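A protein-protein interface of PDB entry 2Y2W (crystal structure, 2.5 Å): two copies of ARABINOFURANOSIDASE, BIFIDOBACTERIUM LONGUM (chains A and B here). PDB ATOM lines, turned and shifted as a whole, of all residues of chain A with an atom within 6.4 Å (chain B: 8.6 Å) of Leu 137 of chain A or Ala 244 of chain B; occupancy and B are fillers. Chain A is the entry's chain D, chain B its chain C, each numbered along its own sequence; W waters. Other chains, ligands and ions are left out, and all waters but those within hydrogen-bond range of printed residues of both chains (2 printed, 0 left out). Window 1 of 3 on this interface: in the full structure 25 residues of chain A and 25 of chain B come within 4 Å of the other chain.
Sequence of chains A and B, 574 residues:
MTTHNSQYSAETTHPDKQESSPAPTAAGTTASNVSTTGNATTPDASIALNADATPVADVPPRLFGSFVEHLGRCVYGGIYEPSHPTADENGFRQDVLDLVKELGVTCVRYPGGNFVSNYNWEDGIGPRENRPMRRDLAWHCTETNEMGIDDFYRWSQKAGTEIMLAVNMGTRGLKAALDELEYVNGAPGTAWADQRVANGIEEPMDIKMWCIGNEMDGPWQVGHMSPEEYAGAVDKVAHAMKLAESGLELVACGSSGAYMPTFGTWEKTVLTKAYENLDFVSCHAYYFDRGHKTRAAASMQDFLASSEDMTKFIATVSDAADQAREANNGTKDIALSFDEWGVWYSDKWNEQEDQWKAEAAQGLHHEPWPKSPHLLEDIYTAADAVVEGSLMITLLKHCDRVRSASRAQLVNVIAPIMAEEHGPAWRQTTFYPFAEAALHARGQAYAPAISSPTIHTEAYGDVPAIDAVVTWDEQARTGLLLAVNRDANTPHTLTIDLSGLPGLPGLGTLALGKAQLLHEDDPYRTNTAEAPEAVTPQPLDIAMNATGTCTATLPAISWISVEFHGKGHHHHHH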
ATOM      1  N   PHE A 115       0.626 -23.789   4.906  1.00  0.00           N
ATOM      2  CA  PHE A 115       1.719 -24.567   5.483  1.00  0.00           C
ATOM      3  C   PHE A 115       2.871 -24.789   4.503  1.00  0.00           C
ATOM      4  O   PHE A 115       4.031 -24.627   4.869  1.00  0.00           O
ATOM      5  CB  PHE A 115       1.183 -25.914   6.008  1.00  0.00           C
ATOM      6  CG  PHE A 115       2.255 -26.883   6.425  1.00  0.00           C
ATOM      7  CD1 PHE A 115       2.896 -26.750   7.653  1.00  0.00           C
ATOM      8  CD2 PHE A 115       2.626 -27.930   5.589  1.00  0.00           C
ATOM      9  CE1 PHE A 115       3.892 -27.651   8.044  1.00  0.00           C
ATOM     10  CE2 PHE A 115       3.621 -28.833   5.969  1.00  0.00           C
ATOM     11  CZ  PHE A 115       4.254 -28.691   7.199  1.00  0.00           C
ATOM     12  N   ASN A 118       6.315 -22.489   3.463  1.00  0.00           N
ATOM     13  CA  ASN A 118       7.576 -22.495   4.206  1.00  0.00           C
ATOM     14  C   ASN A 118       7.938 -23.899   4.695  1.00  0.00           C
ATOM     15  O   ASN A 118       8.357 -24.094   5.837  1.00  0.00           O
ATOM     16  CB  ASN A 118       7.558 -21.463   5.348  1.00  0.00           C
ATOM     17  CG  ASN A 118       6.738 -21.913   6.547  1.00  0.00           C
ATOM     18  OD1 ASN A 118       7.251 -21.975   7.664  1.00  0.00           O
ATOM     19  ND2 ASN A 118       5.466 -22.230   6.324  1.00  0.00           N
ATOM     20  N   ARG A 135       9.666 -25.109  12.442  1.00  0.00           N
ATOM     21  CA  ARG A 135       8.644 -24.093  12.630  1.00  0.00           C
ATOM     22  C   ARG A 135       7.712 -24.071  11.432  1.00  0.00           C
ATOM     23  O   ARG A 135       8.147 -24.277  10.297  1.00  0.00           O
ATOM     24  CB  ARG A 135       9.288 -22.710  12.727  1.00  0.00           C
ATOM     25  CG  ARG A 135       9.820 -22.311  14.077  1.00  0.00           C
ATOM     26  CD  ARG A 135      10.394 -20.906  13.990  1.00  0.00           C
ATOM     27  NE  ARG A 135      10.527 -20.275  15.298  1.00  0.00           N
ATOM     28  CZ  ARG A 135      10.938 -19.027  15.496  1.00  0.00           C
ATOM     29  NH1 ARG A 135      11.269 -18.251  14.465  1.00  0.00           N
ATOM     30  NH2 ARG A 135      11.019 -18.550  16.732  1.00  0.00           N
ATOM     31  N   ASP A 136       6.434 -23.810  11.685  1.00  0.00           N
ATOM     32  CA  ASP A 136       5.521 -23.401  10.629  1.00  0.00           C
ATOM     33  C   ASP A 136       5.085 -21.967  10.888  1.00  0.00           C
ATOM     34  O   ASP A 136       4.443 -21.681  11.897  1.00  0.00           O
ATOM     35  CB  ASP A 136       4.299 -24.318  10.543  1.00  0.00           C
ATOM     36  CG  ASP A 136       3.226 -23.765   9.617  1.00  0.00           C
ATOM     37  OD1 ASP A 136       3.568 -23.361   8.483  1.00  0.00           O
ATOM     38  OD2 ASP A 136       2.045 -23.720  10.027  1.00  0.00           O
ATOM     39  N   LEU A 137       5.442 -21.072   9.971  1.00  0.00           N
ATOM     40  CA  LEU A 137       5.096 -19.655  10.089  1.00  0.00           C
ATOM     41  C   LEU A 137       3.605 -19.389   9.909  1.00  0.00           C
ATOM     42  O   LEU A 137       3.041 -18.539  10.593  1.00  0.00           O
ATOM     43  CB  LEU A 137       5.900 -18.820   9.091  1.00  0.00           C
ATOM     44  CG  LEU A 137       7.205 -18.171   9.559  1.00  0.00           C
ATOM     45  CD1 LEU A 137       8.245 -19.186  10.030  1.00  0.00           C
ATOM     46  CD2 LEU A 137       7.767 -17.312   8.441  1.00  0.00           C
ATOM     47  N   ALA A 138       2.978 -20.124   8.994  1.00  0.00           N
ATOM     48  CA  ALA A 138       1.575 -19.903   8.628  1.00  0.00           C
ATOM     49  C   ALA A 138       0.595 -20.003   9.804  1.00  0.00           C
ATOM     50  O   ALA A 138      -0.281 -19.152   9.957  1.00  0.00           O
ATOM     51  CB  ALA A 138       1.169 -20.853   7.519  1.00  0.00           C
ATOM     52  N   TRP A 139       0.752 -21.035  10.629  1.00  0.00           N
ATOM     53  CA  TRP A 139      -0.176 -21.297  11.733  1.00  0.00           C
ATOM     54  C   TRP A 139       0.485 -21.175  13.107  1.00  0.00           C
ATOM     55  O   TRP A 139      -0.141 -21.451  14.133  1.00  0.00           O
ATOM     56  CB  TRP A 139      -0.854 -22.660  11.542  1.00  0.00           C
ATOM     57  CG  TRP A 139      -1.558 -22.721  10.230  1.00  0.00           C
ATOM     58  CD1 TRP A 139      -1.135 -23.359   9.100  1.00  0.00           C
ATOM     59  CD2 TRP A 139      -2.783 -22.063   9.886  1.00  0.00           C
ATOM     60  NE1 TRP A 139      -2.032 -23.157   8.079  1.00  0.00           N
ATOM     61  CE2 TRP A 139      -3.051 -22.361   8.533  1.00  0.00           C
ATOM     62  CE3 TRP A 139      -3.685 -21.260  10.594  1.00  0.00           C
ATOM     63  CZ2 TRP A 139      -4.189 -21.889   7.872  1.00  0.00           C
ATOM     64  CZ3 TRP A 139      -4.815 -20.787   9.937  1.00  0.00           C
ATOM     65  CH2 TRP A 139      -5.057 -21.105   8.589  1.00  0.00           C
ATOM     66  N   HIS A 140       1.743 -20.737  13.103  1.00  0.00           N
ATOM     67  CA  HIS A 140       2.526 -20.496  14.317  1.00  0.00           C
ATOM     68  C   HIS A 140       2.625 -21.748  15.187  1.00  0.00           C
ATOM     69  O   HIS A 140       2.295 -21.728  16.369  1.00  0.00           O
ATOM     70  CB  HIS A 140       1.964 -19.303  15.103  1.00  0.00           C
ATOM     71  CG  HIS A 140       2.979 -18.606  15.953  1.00  0.00           C
ATOM     72  ND1 HIS A 140       3.980 -17.821  15.421  1.00  0.00           N
ATOM     73  CD2 HIS A 140       3.145 -18.567  17.295  1.00  0.00           C
ATOM     74  CE1 HIS A 140       4.720 -17.332  16.399  1.00  0.00           C
ATOM     75  NE2 HIS A 140       4.234 -17.768  17.547  1.00  0.00           N
ATOM     76  N   CYS A 141       3.081 -22.838  14.581  1.00  0.00           N
ATOM     77  CA  CYS A 141       3.202 -24.113  15.274  1.00  0.00           C
ATOM     78  C   CYS A 141       4.576 -24.723  15.070  1.00  0.00           C
ATOM     79  O   CYS A 141       5.247 -24.435  14.079  1.00  0.00           O
ATOM     80  CB  CYS A 141       2.131 -25.090  14.777  1.00  0.00           C
ATOM     81  SG  CYS A 141       0.436 -24.572  15.125  1.00  0.00           S
ATOM     82  N   VAL A 222       3.478 -16.771   2.772  1.00  0.00           N
ATOM     83  CA  VAL A 222       4.925 -16.631   2.843  1.00  0.00           C
ATOM     84  C   VAL A 222       5.490 -16.591   1.426  1.00  0.00           C
ATOM     85  O   VAL A 222       5.282 -17.516   0.638  1.00  0.00           O
ATOM     86  CB  VAL A 222       5.575 -17.762   3.679  1.00  0.00           C
ATOM     87  CG1 VAL A 222       7.093 -17.612   3.715  1.00  0.00           C
ATOM     88  CG2 VAL A 222       5.018 -17.761   5.091  1.00  0.00           C
ATOM     89  N   TRP A 356      -2.430 -10.812  17.670  1.00  0.00           N
ATOM     90  CA  TRP A 356      -1.022 -11.146  17.458  1.00  0.00           C
ATOM     91  C   TRP A 356      -0.247  -9.935  16.935  1.00  0.00           C
ATOM     92  O   TRP A 356       0.910  -9.727  17.302  1.00  0.00           O
ATOM     93  CB  TRP A 356      -0.911 -12.334  16.489  1.00  0.00           C
ATOM     94  CG  TRP A 356       0.449 -12.547  15.882  1.00  0.00           C
ATOM     95  CD1 TRP A 356       0.827 -12.258  14.601  1.00  0.00           C
ATOM     96  CD2 TRP A 356       1.604 -13.100  16.526  1.00  0.00           C
ATOM     97  NE1 TRP A 356       2.145 -12.593  14.407  1.00  0.00           N
ATOM     98  CE2 TRP A 356       2.648 -13.111  15.572  1.00  0.00           C
ATOM     99  CE3 TRP A 356       1.861 -13.583  17.815  1.00  0.00           C
ATOM    100  CZ2 TRP A 356       3.929 -13.589  15.868  1.00  0.00           C
ATOM    101  CZ3 TRP A 356       3.135 -14.058  18.109  1.00  0.00           C
ATOM    102  CH2 TRP A 356       4.153 -14.055  17.138  1.00  0.00           C
ATOM    103  N   HIS A 365       8.733 -12.870  21.802  1.00  0.00           N
ATOM    104  CA  HIS A 365       8.124 -14.038  22.433  1.00  0.00           C
ATOM    105  C   HIS A 365       9.132 -15.176  22.581  1.00  0.00           C
ATOM    106  O   HIS A 365       9.741 -15.610  21.603  1.00  0.00           O
ATOM    107  CB  HIS A 365       6.898 -14.504  21.642  1.00  0.00           C
ATOM    108  CG  HIS A 365       5.888 -13.424  21.406  1.00  0.00           C
ATOM    109  ND1 HIS A 365       5.753 -12.784  20.192  1.00  0.00           N
ATOM    110  CD2 HIS A 365       4.975 -12.860  22.232  1.00  0.00           C
ATOM    111  CE1 HIS A 365       4.797 -11.877  20.280  1.00  0.00           C
ATOM    112  NE2 HIS A 365       4.308 -11.903  21.506  1.00  0.00           N
ATOM    113  N   TRP A 369       6.479 -22.598  20.191  1.00  0.00           N
ATOM    114  CA  TRP A 369       5.256 -22.630  19.400  1.00  0.00           C
ATOM    115  C   TRP A 369       4.501 -23.935  19.687  1.00  0.00           C
ATOM    116  O   TRP A 369       5.127 -24.978  19.882  1.00  0.00           O
ATOM    117  CB  TRP A 369       5.591 -22.481  17.910  1.00  0.00           C
ATOM    118  CG  TRP A 369       6.309 -21.181  17.549  1.00  0.00           C
ATOM    119  CD1 TRP A 369       6.921 -20.304  18.408  1.00  0.00           C
ATOM    120  CD2 TRP A 369       6.513 -20.648  16.232  1.00  0.00           C
ATOM    121  NE1 TRP A 369       7.472 -19.257  17.709  1.00  0.00           N
ATOM    122  CE2 TRP A 369       7.238 -19.443  16.373  1.00  0.00           C
ATOM    123  CE3 TRP A 369       6.143 -21.066  14.947  1.00  0.00           C
ATOM    124  CZ2 TRP A 369       7.599 -18.651  15.278  1.00  0.00           C
ATOM    125  CZ3 TRP A 369       6.507 -20.277  13.856  1.00  0.00           C
ATOM    126  CH2 TRP A 369       7.226 -19.084  14.032  1.00  0.00           C
ATOM    127  N   LEU B 174      14.988 -15.116   1.384  1.00  0.00           N
ATOM    128  CA  LEU B 174      13.925 -15.398   2.345  1.00  0.00           C
ATOM    129  C   LEU B 174      14.214 -16.586   3.266  1.00  0.00           C
ATOM    130  O   LEU B 174      14.129 -16.459   4.488  1.00  0.00           O
ATOM    131  CB  LEU B 174      12.593 -15.591   1.606  1.00  0.00           C
ATOM    132  CG  LEU B 174      11.296 -15.765   2.401  1.00  0.00           C
ATOM    133  CD1 LEU B 174      10.890 -14.467   3.070  1.00  0.00           C
ATOM    134  CD2 LEU B 174      10.180 -16.259   1.487  1.00  0.00           C
ATOM    135  N   ALA B 177      17.128 -16.095   5.826  1.00  0.00           N
ATOM    136  CA  ALA B 177      16.783 -15.102   6.841  1.00  0.00           C
ATOM    137  C   ALA B 177      15.908 -15.718   7.930  1.00  0.00           C
ATOM    138  O   ALA B 177      16.178 -15.544   9.120  1.00  0.00           O
ATOM    139  CB  ALA B 177      16.100 -13.895   6.210  1.00  0.00           C
ATOM    140  N   LEU B 178      14.879 -16.453   7.512  1.00  0.00           N
ATOM    141  CA  LEU B 178      14.001 -17.170   8.434  1.00  0.00           C
ATOM    142  C   LEU B 178      14.754 -18.235   9.229  1.00  0.00           C
ATOM    143  O   LEU B 178      14.452 -18.469  10.402  1.00  0.00           O
ATOM    144  CB  LEU B 178      12.827 -17.805   7.683  1.00  0.00           C
ATOM    145  CG  LEU B 178      11.872 -16.867   6.941  1.00  0.00           C
ATOM    146  CD1 LEU B 178      10.816 -17.664   6.182  1.00  0.00           C
ATOM    147  CD2 LEU B 178      11.223 -15.862   7.884  1.00  0.00           C
ATOM    148  N   ASP B 179      15.727 -18.874   8.581  1.00  0.00           N
ATOM    149  CA  ASP B 179      16.588 -19.855   9.241  1.00  0.00           C
ATOM    150  C   ASP B 179      17.417 -19.211  10.359  1.00  0.00           C
ATOM    151  O   ASP B 179      17.516 -19.763  11.457  1.00  0.00           O
ATOM    152  CB  ASP B 179      17.502 -20.549   8.224  1.00  0.00           C
ATOM    153  CG  ASP B 179      16.794 -21.653   7.446  1.00  0.00           C
ATOM    154  OD1 ASP B 179      15.683 -22.065   7.849  1.00  0.00           O
ATOM    155  OD2 ASP B 179      17.357 -22.119   6.429  1.00  0.00           O
ATOM    156  N   LEU B 181      16.789 -16.266  11.855  1.00  0.00           N
ATOM    157  CA  LEU B 181      15.855 -15.761  12.858  1.00  0.00           C
ATOM    158  C   LEU B 181      15.511 -16.833  13.889  1.00  0.00           C
ATOM    159  O   LEU B 181      15.536 -16.569  15.090  1.00  0.00           O
ATOM    160  CB  LEU B 181      14.579 -15.224  12.195  1.00  0.00           C
ATOM    161  CG  LEU B 181      13.404 -14.817  13.093  1.00  0.00           C
ATOM    162  CD1 LEU B 181      13.752 -13.630  13.979  1.00  0.00           C
ATOM    163  CD2 LEU B 181      12.178 -14.509  12.254  1.00  0.00           C
ATOM    164  N   GLU B 182      15.202 -18.034  13.405  1.00  0.00           N
ATOM    165  CA  GLU B 182      14.869 -19.177  14.254  1.00  0.00           C
ATOM    166  C   GLU B 182      16.050 -19.610  15.133  1.00  0.00           C
ATOM    167  O   GLU B 182      15.875 -19.879  16.326  1.00  0.00           O
ATOM    168  CB  GLU B 182      14.391 -20.348  13.387  1.00  0.00           C
ATOM    169  CG  GLU B 182      13.913 -21.573  14.162  1.00  0.00           C
ATOM    170  CD  GLU B 182      13.488 -22.725  13.257  1.00  0.00           C
ATOM    171  OE1 GLU B 182      12.915 -22.478  12.169  1.00  0.00           O
ATOM    172  OE2 GLU B 182      13.733 -23.887  13.636  1.00  0.00           O
ATOM    173  N   ASN B 185      16.767 -16.516  17.739  1.00  0.00           N
ATOM    174  CA  ASN B 185      15.747 -16.162  18.721  1.00  0.00           C
ATOM    175  C   ASN B 185      14.881 -17.321  19.238  1.00  0.00           C
ATOM    176  O   ASN B 185      14.132 -17.154  20.201  1.00  0.00           O
ATOM    177  CB  ASN B 185      14.859 -15.045  18.167  1.00  0.00           C
ATOM    178  CG  ASN B 185      15.544 -13.687  18.178  1.00  0.00           C
ATOM    179  OD1 ASN B 185      16.551 -13.486  18.859  1.00  0.00           O
ATOM    180  ND2 ASN B 185      14.992 -12.745  17.425  1.00  0.00           N
ATOM    181  N   LYS B 236       8.348  -9.677   0.769  1.00  0.00           N
ATOM    182  CA  LYS B 236       8.368 -11.089   1.141  1.00  0.00           C
ATOM    183  C   LYS B 236       9.058 -11.324   2.485  1.00  0.00           C
ATOM    184  O   LYS B 236       8.511 -12.002   3.353  1.00  0.00           O
ATOM    185  CB  LYS B 236       9.047 -11.919   0.047  1.00  0.00           C
ATOM    186  CG  LYS B 236       8.270 -11.979  -1.254  1.00  0.00           C
ATOM    187  CD  LYS B 236       9.125 -12.517  -2.390  1.00  0.00           C
ATOM    188  CE  LYS B 236       8.440 -12.310  -3.731  1.00  0.00           C
ATOM    189  NZ  LYS B 236       8.325 -10.862  -4.085  1.00  0.00           N
ATOM    190  N   VAL B 237      10.248 -10.751   2.655  1.00  0.00           N
ATOM    191  CA  VAL B 237      11.031 -10.941   3.882  1.00  0.00           C
ATOM    192  C   VAL B 237      10.371 -10.300   5.108  1.00  0.00           C
ATOM    193  O   VAL B 237      10.238 -10.949   6.147  1.00  0.00           O
ATOM    194  CB  VAL B 237      12.507 -10.478   3.715  1.00  0.00           C
ATOM    195  CG1 VAL B 237      13.254 -10.549   5.040  1.00  0.00           C
ATOM    196  CG2 VAL B 237      13.216 -11.335   2.679  1.00  0.00           C
ATOM    197  N   ALA B 238       9.950  -9.044   4.974  1.00  0.00           N
ATOM    198  CA  ALA B 238       9.287  -8.323   6.067  1.00  0.00           C
ATOM    199  C   ALA B 238       8.012  -9.012   6.550  1.00  0.00           C
ATOM    200  O   ALA B 238       7.819  -9.183   7.759  1.00  0.00           O
ATOM    201  CB  ALA B 238       8.998  -6.877   5.670  1.00  0.00           C
ATOM    202  N   HIS B 239       7.151  -9.409   5.613  1.00  0.00           N
ATOM    203  CA  HIS B 239       5.923 -10.120   5.966  1.00  0.00           C
ATOM    204  C   HIS B 239       6.211 -11.414   6.726  1.00  0.00           C
ATOM    205  O   HIS B 239       5.622 -11.665   7.779  1.00  0.00           O
ATOM    206  CB  HIS B 239       5.066 -10.417   4.737  1.00  0.00           C
ATOM    207  CG  HIS B 239       4.025 -11.464   4.982  1.00  0.00           C
ATOM    208  ND1 HIS B 239       4.201 -12.784   4.624  1.00  0.00           N
ATOM    209  CD2 HIS B 239       2.817 -11.396   5.590  1.00  0.00           C
ATOM    210  CE1 HIS B 239       3.137 -13.479   4.984  1.00  0.00           C
ATOM    211  NE2 HIS B 239       2.283 -12.661   5.573  1.00  0.00           N
ATOM    212  N   ALA B 240       7.118 -12.226   6.184  1.00  0.00           N
ATOM    213  CA  ALA B 240       7.476 -13.512   6.782  1.00  0.00           C
ATOM    214  C   ALA B 240       8.030 -13.370   8.200  1.00  0.00           C
ATOM    215  O   ALA B 240       7.579 -14.062   9.112  1.00  0.00           O
ATOM    216  CB  ALA B 240       8.459 -14.253   5.896  1.00  0.00           C
ATOM    217  N   MET B 241       8.989 -12.467   8.384  1.00  0.00           N
ATOM    218  CA  MET B 241       9.637 -12.281   9.689  1.00  0.00           C
ATOM    219  C   MET B 241       8.697 -11.712  10.755  1.00  0.00           C
ATOM    220  O   MET B 241       8.836 -12.019  11.936  1.00  0.00           O
ATOM    221  CB  MET B 241      10.892 -11.416   9.558  1.00  0.00           C
ATOM    222  CG  MET B 241      11.969 -12.042   8.684  1.00  0.00           C
ATOM    223  SD  MET B 241      13.500 -11.100   8.657  1.00  0.00           S
ATOM    224  CE  MET B 241      14.218 -11.562  10.232  1.00  0.00           C
ATOM    225  N   LYS B 242       7.742 -10.890  10.328  1.00  0.00           N
ATOM    226  CA  LYS B 242       6.735 -10.346  11.233  1.00  0.00           C
ATOM    227  C   LYS B 242       5.701 -11.401  11.611  1.00  0.00           C
ATOM    228  O   LYS B 242       5.139 -11.364  12.705  1.00  0.00           O
ATOM    229  CB  LYS B 242       6.047  -9.135  10.607  1.00  0.00           C
ATOM    230  CG  LYS B 242       6.850  -7.849  10.703  1.00  0.00           C
ATOM    231  CD  LYS B 242       6.598  -7.131  12.017  1.00  0.00           C
ATOM    232  CE  LYS B 242       7.348  -5.818  12.065  1.00  0.00           C
ATOM    233  NZ  LYS B 242       7.011  -5.061  13.292  1.00  0.00           N
ATOM    234  N   LEU B 243       5.453 -12.334  10.697  1.00  0.00           N
ATOM    235  CA  LEU B 243       4.533 -13.437  10.945  1.00  0.00           C
ATOM    236  C   LEU B 243       5.094 -14.394  11.994  1.00  0.00           C
ATOM    237  O   LEU B 243       4.356 -14.885  12.848  1.00  0.00           O
ATOM    238  CB  LEU B 243       4.221 -14.176   9.639  1.00  0.00           C
ATOM    239  CG  LEU B 243       3.129 -15.252   9.625  1.00  0.00           C
ATOM    240  CD1 LEU B 243       1.754 -14.690  10.003  1.00  0.00           C
ATOM    241  CD2 LEU B 243       3.081 -15.917   8.252  1.00  0.00           C
ATOM    242  N   ALA B 244       6.400 -14.643  11.930  1.00  0.00           N
ATOM    243  CA  ALA B 244       7.081 -15.494  12.904  1.00  0.00           C
ATOM    244  C   ALA B 244       7.264 -14.794  14.250  1.00  0.00           C
ATOM    245  O   ALA B 244       7.234 -15.438  15.303  1.00  0.00           O
ATOM    246  CB  ALA B 244       8.425 -15.954  12.359  1.00  0.00           C
ATOM    247  N   GLU B 245       7.457 -13.478  14.205  1.00  0.00           N
ATOM    248  CA  GLU B 245       7.679 -12.677  15.402  1.00  0.00           C
ATOM    249  C   GLU B 245       7.218 -11.241  15.170  1.00  0.00           C
ATOM    250  O   GLU B 245       7.891 -10.464  14.487  1.00  0.00           O
ATOM    251  CB  GLU B 245       9.159 -12.715  15.810  1.00  0.00           C
ATOM    252  CG  GLU B 245       9.507 -11.859  17.025  1.00  0.00           C
ATOM    253  CD  GLU B 245       8.901 -12.384  18.311  1.00  0.00           C
ATOM    254  OE1 GLU B 245       9.427 -13.384  18.847  1.00  0.00           O
ATOM    255  OE2 GLU B 245       7.908 -11.791  18.793  1.00  0.00           O
ATOM    256  N   SER B 246       6.071 -10.898  15.750  1.00  0.00           N
ATOM    257  CA  SER B 246       5.473  -9.575  15.579  1.00  0.00           C
ATOM    258  C   SER B 246       6.219  -8.480  16.337  1.00  0.00           C
ATOM    259  O   SER B 246       6.063  -7.297  16.030  1.00  0.00           O
ATOM    260  CB  SER B 246       4.005  -9.595  16.001  1.00  0.00           C
ATOM    261  OG  SER B 246       3.878  -9.971  17.359  1.00  0.00           O
ATOM    262  N   GLY B 247       7.027  -8.877  17.317  1.00  0.00           N
ATOM    263  CA  GLY B 247       7.788  -7.929  18.131  1.00  0.00           C
ATOM    264  C   GLY B 247       9.065  -7.403  17.494  1.00  0.00           C
ATOM    265  O   GLY B 247       9.808  -6.652  18.124  1.00  0.00           O
ATOM    266  N   LEU B 248       9.326  -7.794  16.249  1.00  0.00           N
ATOM    267  CA  LEU B 248      10.532  -7.370  15.539  1.00  0.00           C
ATOM    268  C   LEU B 248      10.441  -5.929  15.045  1.00  0.00           C
ATOM    269  O   LEU B 248       9.352  -5.407  14.800  1.00  0.00           O
ATOM    270  CB  LEU B 248      10.825  -8.303  14.358  1.00  0.00           C
ATOM    271  CG  LEU B 248      11.228  -9.755  14.628  1.00  0.00           C
ATOM    272  CD1 LEU B 248      11.473 -10.471  13.314  1.00  0.00           C
ATOM    273  CD2 LEU B 248      12.456  -9.860  15.528  1.00  0.00           C
HETATM  274  O   HOH W   1      11.927 -17.988  11.127  1.00  0.00           O
HETATM  275  O   HOH W   2       4.026 -17.425  12.715  1.00  0.00           O
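The side-chain hydroxyl of Ser 246 of chain B lies within hydrogen-bond range of the backbone carbonyl oxygen of Trp 356 of chain A, 3.0 Å away. ND1 of His 365 of chain A is in hydrogen-bond range of OE2 of Glu 245 of chain B, at 2.8 Å.
Water W2 lies within hydrogen-bond range of O of Leu 243 of chain B, O of Leu 137 of chain A and ND1 of His 140 of chain A. Water W1 bridges the backbone carbonyl oxygen (O) of Leu 178 of chain B and the guanidinium group (NH1) of Arg 135 of chain A.
OD1 of Asn 118 of chain A lies within hydrogen-bond range of N of Leu 137 of chain A (3.1 Å). N of Gly 247 of chain B lies close to OE2 of Glu 245 of chain B (3.4 Å). The side-chain amino group of Lys 242 of chain B is in hydrogen-bond range of the backbone carbonyl oxygen of Leu 248 of chain B (2.8 Å).
Of the 20 printed residues of chain B, 9 touch a printed residue of chain A. Among the printed residues, 16 pairs touch across the chains.
No position is printed for both chains. Of the 16 pairs that touch across the chains among the printed residues, none has its exchanged pair printed and touching as well.
Asn 118 of chain A touches none of the printed residues of chain B. No residue of chain B comes within 4 Å of Asp 136 of chain A. Leu 137 of chain A touches just these residues of chain B: Leu 178, Ala 240, Leu 243 and Ala 244. Printed residues of chain B within 4 Å of His 140 of chain A: Leu 243 (3.9 Å) and Ala 244 (3.3 Å). Of the printed residues of chain B, Val 222 of chain A touches His 239. Lys 236 of chain B touches none of the printed residues of chain A. Printed residues of chain A within 4 Å of Lys 242 of chain B: Trp 356 (3.7 Å). Of chain A, only Leu 137, His 140, Trp 356 and Trp 369 come within 4 Å of Ala 244 of chain B. Of the printed residues of chain A, Ser 246 of chain B touches Trp 356 and His 365. The nearest residue of chain B that does not touch Leu 137 of chain A is Met 241 of chain B (5.0 Å). The nearest residue of chain A that does not touch Ala 244 of chain B is Arg 135 of chain A (4.2 Å).
Among the printed residues, pairs that only touch across the chains: Trp 369 of chain A with Ala 244 of chain B, Trp 356 of chain A with Leu 243 of chain B, Leu 137 of chain A with Ala 240 of chain B, His 140 of chain A with Ala 244 of chain B, Leu 137 of chain A with Leu 243 of chain B, Arg 135 of chain A with Glu 182 of chain B, His 365 of chain A with Ser 246 of chain B, Trp 356 of chain A with Lys 242 of chain B, Leu 137 of chain A with Ala 244 of chain B, Leu 137 of chain A with Leu 178 of chain B, Trp 356 of chain A with Ala 244 of chain B, Trp 356 of chain A with Glu 245 of chain B, His 140 of chain A with Leu 243 of chain B and Val 222 of chain A with His 239 of chain B.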
